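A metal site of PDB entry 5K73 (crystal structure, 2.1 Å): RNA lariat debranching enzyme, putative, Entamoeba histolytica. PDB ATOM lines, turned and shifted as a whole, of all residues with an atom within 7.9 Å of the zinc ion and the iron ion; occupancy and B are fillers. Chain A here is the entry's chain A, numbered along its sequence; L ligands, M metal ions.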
ATOM      1  N   GLY A  15      31.476   3.509 -24.855  1.00  0.00           N
ATOM      2  CA  GLY A  15      30.766   2.308 -25.247  1.00  0.00           C
ATOM      3  C   GLY A  15      29.497   2.082 -24.453  1.00  0.00           C
ATOM      4  O   GLY A  15      28.525   2.825 -24.607  1.00  0.00           O
ATOM      5  N   CYS A  16      29.483   1.060 -23.604  1.00  0.00           N
ATOM      6  CA  CYS A  16      28.325   0.733 -22.778  1.00  0.00           C
ATOM      7  C   CYS A  16      28.462   1.386 -21.409  1.00  0.00           C
ATOM      8  O   CYS A  16      29.516   1.287 -20.771  1.00  0.00           O
ATOM      9  CB  CYS A  16      28.180  -0.773 -22.629  1.00  0.00           C
ATOM     10  SG  CYS A  16      27.899  -1.674 -24.171  1.00  0.00           S
ATOM     11  N   VAL A  17      27.403   2.055 -20.962  1.00  0.00           N
ATOM     12  CA  VAL A  17      27.395   2.683 -19.646  1.00  0.00           C
ATOM     13  C   VAL A  17      26.865   1.725 -18.585  1.00  0.00           C
ATOM     14  O   VAL A  17      27.460   1.572 -17.521  1.00  0.00           O
ATOM     15  CB  VAL A  17      26.583   3.992 -19.682  1.00  0.00           C
ATOM     16  CG1 VAL A  17      26.276   4.463 -18.271  1.00  0.00           C
ATOM     17  CG2 VAL A  17      27.357   5.054 -20.433  1.00  0.00           C
ATOM     18  N   HIS A  18      25.735   1.071 -18.875  1.00  0.00           N
ATOM     19  CA  HIS A  18      25.102   0.120 -17.955  1.00  0.00           C
ATOM     20  C   HIS A  18      24.809   0.763 -16.597  1.00  0.00           C
ATOM     21  O   HIS A  18      24.998   0.149 -15.545  1.00  0.00           O
ATOM     22  CB  HIS A  18      25.943  -1.138 -17.787  1.00  0.00           C
ATOM     23  CG  HIS A  18      25.930  -2.034 -18.989  1.00  0.00           C
ATOM     24  ND1 HIS A  18      24.821  -2.751 -19.372  1.00  0.00           N
ATOM     25  CD2 HIS A  18      26.892  -2.319 -19.895  1.00  0.00           C
ATOM     26  CE1 HIS A  18      25.090  -3.443 -20.464  1.00  0.00           C
ATOM     27  NE2 HIS A  18      26.345  -3.201 -20.802  1.00  0.00           N
ATOM     28  N   THR A  45      27.292   5.003 -26.932  1.00  0.00           N
ATOM     29  CA  THR A  45      26.719   4.067 -27.899  1.00  0.00           C
ATOM     30  C   THR A  45      25.563   3.247 -27.359  1.00  0.00           C
ATOM     31  O   THR A  45      25.001   2.442 -28.118  1.00  0.00           O
ATOM     32  CB  THR A  45      27.802   3.129 -28.434  1.00  0.00           C
ATOM     33  OG1 THR A  45      28.397   2.409 -27.346  1.00  0.00           O
ATOM     34  CG2 THR A  45      28.882   3.912 -29.167  1.00  0.00           C
ATOM     35  N   GLY A  46      25.184   3.391 -26.101  1.00  0.00           N
ATOM     36  CA  GLY A  46      23.957   2.785 -25.635  1.00  0.00           C
ATOM     37  C   GLY A  46      24.114   2.076 -24.301  1.00  0.00           C
ATOM     38  O   GLY A  46      25.134   2.220 -23.628  1.00  0.00           O
ATOM     39  N   ASP A  47      23.087   1.313 -23.963  1.00  0.00           N
ATOM     40  CA  ASP A  47      22.937   0.684 -22.646  1.00  0.00           C
ATOM     41  C   ASP A  47      22.984   1.735 -21.539  1.00  0.00           C
ATOM     42  O   ASP A  47      23.783   1.670 -20.596  1.00  0.00           O
ATOM     43  CB  ASP A  47      23.980  -0.415 -22.430  1.00  0.00           C
ATOM     44  CG  ASP A  47      23.685  -1.656 -23.253  1.00  0.00           C
ATOM     45  OD1 ASP A  47      22.564  -1.750 -23.805  1.00  0.00           O
ATOM     46  OD2 ASP A  47      24.562  -2.540 -23.352  1.00  0.00           O
ATOM     47  N   GLN A  49      20.283   2.677 -19.549  1.00  0.00           N
ATOM     48  CA  GLN A  49      19.446   2.301 -18.408  1.00  0.00           C
ATOM     49  C   GLN A  49      18.917   3.544 -17.683  1.00  0.00           C
ATOM     50  O   GLN A  49      19.156   3.762 -16.497  1.00  0.00           O
ATOM     51  CB  GLN A  49      20.216   1.403 -17.438  1.00  0.00           C
ATOM     52  CG  GLN A  49      20.833   0.171 -18.081  1.00  0.00           C
ATOM     53  CD  GLN A  49      21.466  -0.767 -17.073  1.00  0.00           C
ATOM     54  OE1 GLN A  49      21.261  -0.615 -15.871  1.00  0.00           O
ATOM     55  NE2 GLN A  49      22.220  -1.735 -17.555  1.00  0.00           N
ATOM     56  N   GLY A  90      20.020   4.271 -27.915  1.00  0.00           N
ATOM     57  CA  GLY A  90      19.588   3.171 -27.090  1.00  0.00           C
ATOM     58  C   GLY A  90      20.297   1.872 -27.432  1.00  0.00           C
ATOM     59  O   GLY A  90      20.671   1.637 -28.584  1.00  0.00           O
ATOM     60  N   GLY A  91      20.484   1.034 -26.417  1.00  0.00           N
ATOM     61  CA  GLY A  91      21.059  -0.278 -26.625  1.00  0.00           C
ATOM     62  C   GLY A  91      20.047  -1.378 -26.409  1.00  0.00           C
ATOM     63  O   GLY A  91      18.898  -1.261 -26.839  1.00  0.00           O
ATOM     64  N   ASN A  92      20.460  -2.465 -25.741  1.00  0.00           N
ATOM     65  CA  ASN A  92      19.551  -3.539 -25.373  1.00  0.00           C
ATOM     66  C   ASN A  92      19.241  -3.573 -23.883  1.00  0.00           C
ATOM     67  O   ASN A  92      18.330  -4.308 -23.480  1.00  0.00           O
ATOM     68  CB  ASN A  92      20.114  -4.899 -25.824  1.00  0.00           C
ATOM     69  CG  ASN A  92      21.500  -5.166 -25.262  1.00  0.00           C
ATOM     70  OD1 ASN A  92      22.487  -4.585 -25.720  1.00  0.00           O
ATOM     71  ND2 ASN A  92      21.584  -6.059 -24.283  1.00  0.00           N
ATOM     72  N   HIS A  93      19.955  -2.809 -23.075  1.00  0.00           N
ATOM     73  CA  HIS A  93      19.664  -2.658 -21.641  1.00  0.00           C
ATOM     74  C   HIS A  93      19.209  -1.218 -21.420  1.00  0.00           C
ATOM     75  O   HIS A  93      20.027  -0.323 -21.182  1.00  0.00           O
ATOM     76  CB  HIS A  93      20.885  -3.001 -20.793  1.00  0.00           C
ATOM     77  CG  HIS A  93      21.201  -4.459 -20.763  1.00  0.00           C
ATOM     78  ND1 HIS A  93      22.250  -4.972 -20.027  1.00  0.00           N
ATOM     79  CD2 HIS A  93      20.612  -5.516 -21.360  1.00  0.00           C
ATOM     80  CE1 HIS A  93      22.292  -6.282 -20.181  1.00  0.00           C
ATOM     81  NE2 HIS A  93      21.313  -6.635 -20.984  1.00  0.00           N
ATOM     82  N   GLU A  94      17.907  -0.994 -21.518  1.00  0.00           N
ATOM     83  CA  GLU A  94      17.344   0.349 -21.434  1.00  0.00           C
ATOM     84  C   GLU A  94      16.017   0.311 -20.686  1.00  0.00           C
ATOM     85  O   GLU A  94      15.361  -0.729 -20.582  1.00  0.00           O
ATOM     86  CB  GLU A  94      17.099   0.952 -22.833  1.00  0.00           C
ATOM     87  CG  GLU A  94      18.297   0.922 -23.774  1.00  0.00           C
ATOM     88  CD  GLU A  94      19.356   1.957 -23.428  1.00  0.00           C
ATOM     89  OE1 GLU A  94      19.144   2.745 -22.480  1.00  0.00           O
ATOM     90  OE2 GLU A  94      20.391   1.979 -24.112  1.00  0.00           O
ATOM     91  N   GLY A 133      19.232   0.478 -30.754  1.00  0.00           N
ATOM     92  CA  GLY A 133      18.791  -0.908 -30.693  1.00  0.00           C
ATOM     93  C   GLY A 133      19.814  -1.910 -31.193  1.00  0.00           C
ATOM     94  O   GLY A 133      20.897  -1.569 -31.696  1.00  0.00           O
ATOM     95  N   ILE A 134      19.453  -3.183 -31.049  1.00  0.00           N
ATOM     96  CA  ILE A 134      20.225  -4.289 -31.594  1.00  0.00           C
ATOM     97  C   ILE A 134      19.322  -5.065 -32.540  1.00  0.00           C
ATOM     98  O   ILE A 134      18.099  -4.975 -32.488  1.00  0.00           O
ATOM     99  CB  ILE A 134      20.803  -5.219 -30.509  1.00  0.00           C
ATOM    100  CG1 ILE A 134      19.684  -5.917 -29.735  1.00  0.00           C
ATOM    101  CG2 ILE A 134      21.710  -4.431 -29.567  1.00  0.00           C
ATOM    102  CD1 ILE A 134      20.182  -7.014 -28.814  1.00  0.00           C
ATOM    103  N   HIS A 182      24.589   0.630 -31.703  1.00  0.00           N
ATOM    104  CA  HIS A 182      24.942  -0.118 -30.512  1.00  0.00           C
ATOM    105  C   HIS A 182      25.700  -1.396 -30.864  1.00  0.00           C
ATOM    106  O   HIS A 182      26.872  -1.550 -30.491  1.00  0.00           O
ATOM    107  CB  HIS A 182      23.699  -0.447 -29.677  1.00  0.00           C
ATOM    108  CG  HIS A 182      24.033  -0.991 -28.321  1.00  0.00           C
ATOM    109  ND1 HIS A 182      24.739  -0.265 -27.384  1.00  0.00           N
ATOM    110  CD2 HIS A 182      23.804  -2.203 -27.758  1.00  0.00           C
ATOM    111  CE1 HIS A 182      24.900  -0.991 -26.298  1.00  0.00           C
ATOM    112  NE2 HIS A 182      24.352  -2.172 -26.498  1.00  0.00           N
ATOM    113  N   ASP A 183      25.062  -2.316 -31.573  1.00  0.00           N
ATOM    114  CA  ASP A 183      25.795  -3.466 -32.071  1.00  0.00           C
ATOM    115  C   ASP A 183      26.524  -3.092 -33.364  1.00  0.00           C
ATOM    116  O   ASP A 183      26.235  -2.083 -34.015  1.00  0.00           O
ATOM    117  CB  ASP A 183      24.858  -4.659 -32.298  1.00  0.00           C
ATOM    118  CG  ASP A 183      23.646  -4.314 -33.130  1.00  0.00           C
ATOM    119  OD1 ASP A 183      23.364  -3.116 -33.341  1.00  0.00           O
ATOM    120  OD2 ASP A 183      22.952  -5.252 -33.577  1.00  0.00           O
ATOM    121  N   GLY A 231      29.262  -0.199 -29.696  1.00  0.00           N
ATOM    122  CA  GLY A 231      29.618  -0.793 -28.415  1.00  0.00           C
ATOM    123  C   GLY A 231      29.157  -2.236 -28.304  1.00  0.00           C
ATOM    124  O   GLY A 231      29.524  -3.067 -29.131  1.00  0.00           O
ATOM    125  N   HIS A 232      28.378  -2.528 -27.266  1.00  0.00           N
ATOM    126  CA  HIS A 232      27.671  -3.797 -27.102  1.00  0.00           C
ATOM    127  C   HIS A 232      28.578  -4.976 -26.773  1.00  0.00           C
ATOM    128  O   HIS A 232      28.297  -5.732 -25.837  1.00  0.00           O
ATOM    129  CB  HIS A 232      26.836  -4.110 -28.348  1.00  0.00           C
ATOM    130  CG  HIS A 232      25.948  -5.302 -28.215  1.00  0.00           C
ATOM    131  ND1 HIS A 232      24.946  -5.383 -27.269  1.00  0.00           N
ATOM    132  CD2 HIS A 232      25.911  -6.470 -28.906  1.00  0.00           C
ATOM    133  CE1 HIS A 232      24.323  -6.543 -27.393  1.00  0.00           C
ATOM    134  NE2 HIS A 232      24.890  -7.218 -28.372  1.00  0.00           N
ATOM    135  N   MET A 233      29.676  -5.143 -27.515  1.00  0.00           N
ATOM    136  CA  MET A 233      30.482  -6.361 -27.437  1.00  0.00           C
ATOM    137  C   MET A 233      31.488  -6.350 -26.294  1.00  0.00           C
ATOM    138  O   MET A 233      32.202  -7.348 -26.126  1.00  0.00           O
ATOM    139  CB  MET A 233      31.201  -6.598 -28.763  1.00  0.00           C
ATOM    140  CG  MET A 233      30.266  -6.663 -29.969  1.00  0.00           C
ATOM    141  SD  MET A 233      29.149  -8.080 -29.962  1.00  0.00           S
ATOM    142  CE  MET A 233      30.248  -9.392 -30.475  1.00  0.00           C
ATOM    143  N   HIS A 234      31.581  -5.268 -25.519  1.00  0.00           N
ATOM    144  CA  HIS A 234      32.421  -5.202 -24.331  1.00  0.00           C
ATOM    145  C   HIS A 234      33.892  -5.466 -24.657  1.00  0.00           C
ATOM    146  O   HIS A 234      34.602  -6.160 -23.926  1.00  0.00           O
ATOM    147  CB  HIS A 234      31.941  -6.168 -23.244  1.00  0.00           C
ATOM    148  CG  HIS A 234      30.539  -5.896 -22.786  1.00  0.00           C
ATOM    149  ND1 HIS A 234      29.828  -6.786 -22.008  1.00  0.00           N
ATOM    150  CD2 HIS A 234      29.725  -4.833 -22.990  1.00  0.00           C
ATOM    151  CE1 HIS A 234      28.624  -6.287 -21.754  1.00  0.00           C
ATOM    152  NE2 HIS A 234      28.537  -5.108 -22.339  1.00  0.00           N
ATOM    153  N   LEU A 249      33.898   0.075 -28.711  1.00  0.00           N
ATOM    154  CA  LEU A 249      34.279   0.405 -27.357  1.00  0.00           C
ATOM    155  C   LEU A 249      33.664  -0.589 -26.377  1.00  0.00           C
ATOM    156  O   LEU A 249      32.649  -1.231 -26.667  1.00  0.00           O
ATOM    157  CB  LEU A 249      33.853   1.837 -26.992  1.00  0.00           C
ATOM    158  CG  LEU A 249      34.267   2.930 -27.973  1.00  0.00           C
ATOM    159  CD1 LEU A 249      33.498   4.213 -27.723  1.00  0.00           C
ATOM    160  CD2 LEU A 249      35.770   3.186 -27.880  1.00  0.00           C
ATOM    161  N   GLY A 250      34.283  -0.696 -25.204  1.00  0.00           N
ATOM    162  CA  GLY A 250      33.838  -1.611 -24.169  1.00  0.00           C
ATOM    163  C   GLY A 250      32.825  -0.987 -23.228  1.00  0.00           C
ATOM    164  O   GLY A 250      32.162   0.007 -23.547  1.00  0.00           O
ATOM    165  N   LYS A 251      32.687  -1.581 -22.049  1.00  0.00           N
ATOM    166  CA  LYS A 251      31.720  -1.147 -21.056  1.00  0.00           C
ATOM    167  C   LYS A 251      32.408  -0.386 -19.930  1.00  0.00           C
ATOM    168  O   LYS A 251      33.559  -0.668 -19.572  1.00  0.00           O
ATOM    169  CB  LYS A 251      30.952  -2.354 -20.488  1.00  0.00           C
ATOM    170  CG  LYS A 251      31.832  -3.371 -19.770  1.00  0.00           C
ATOM    171  CD  LYS A 251      31.058  -4.625 -19.408  1.00  0.00           C
ATOM    172  CE  LYS A 251      29.905  -4.339 -18.459  1.00  0.00           C
ATOM    173  NZ  LYS A 251      29.176  -5.573 -18.085  1.00  0.00           N
ATOM    174  N   ILE A 252      31.685   0.592 -19.381  1.00  0.00           N
ATOM    175  CA  ILE A 252      32.225   1.402 -18.295  1.00  0.00           C
ATOM    176  C   ILE A 252      32.634   0.506 -17.135  1.00  0.00           C
ATOM    177  O   ILE A 252      31.921  -0.444 -16.766  1.00  0.00           O
ATOM    178  CB  ILE A 252      31.192   2.452 -17.854  1.00  0.00           C
ATOM    179  CG1 ILE A 252      31.069   3.549 -18.912  1.00  0.00           C
ATOM    180  CG2 ILE A 252      31.568   3.062 -16.513  1.00  0.00           C
ATOM    181  CD1 ILE A 252      32.342   4.362 -19.104  1.00  0.00           C
HETATM  182  O1  LIG L   1      26.243  -5.397 -23.752  1.00  0.00           O
HETATM  183 ZN    ZN M   1      26.934  -3.536 -22.987  1.00  0.00          ZN
HETATM  184 FE    FE M   2      24.541  -3.950 -25.282  1.00  0.00          FE
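The zinc ion is bound by an oxygen (O1) of the ligand (2.1 Å), a ring nitrogen (NE2) of His 18 (2.3 Å), a ring nitrogen (NE2) of His 234 (2.3 Å), the side-chain sulfur (SG) of Cys 16 (2.4 Å) and the side-chain carboxylate (OD2) of Asp 47 (2.6 Å).
Of the 25 residues printed, 5 come within 4 Å of the zinc ion.
The side-chain amide nitrogen (ND2) of Asn 92 lies close to a ring nitrogen (NE2) of His 93 (3.4 Å). N of Asp 47 sits at hydrogen-bond distance from OE2 of Glu 94 (2.8 Å). The backbone carbonyl oxygen of His 182 sits at hydrogen-bond distance from the backbone NH of Gly 231 (2.9 Å). The backbone NH (N) of Ile 252 is in hydrogen-bond range of the backbone carbonyl oxygen (O) of Cys 16 (2.7 Å). The backbone NH of Cys 16 is in hydrogen-bond range of the backbone carbonyl oxygen of Gly 250, at 2.9 Å. N of His 232 sits close to SG of Cys 16 (3.2 Å). A ring nitrogen (ND1) of His 18 lies within hydrogen-bond range of the side-chain amide nitrogen (NE2) of Gln 49, 3.3 Å away. A ring nitrogen (ND1) of His 182 is in hydrogen-bond range of the backbone carbonyl oxygen of Thr 45, at 2.8 Å.
Of the 25 residues printed, 4 come within 4 Å of the iron ion.
The iron ion is bound by NE2 of His 182 (2.2 Å), OD1 of Asn 92 (2.2 Å), OD2 of Asp 47 (2.4 Å) and ND1 of His 232 (2.5 Å). Slightly farther from the iron ion lies an oxygen (O1) of the ligand (2.7 Å).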
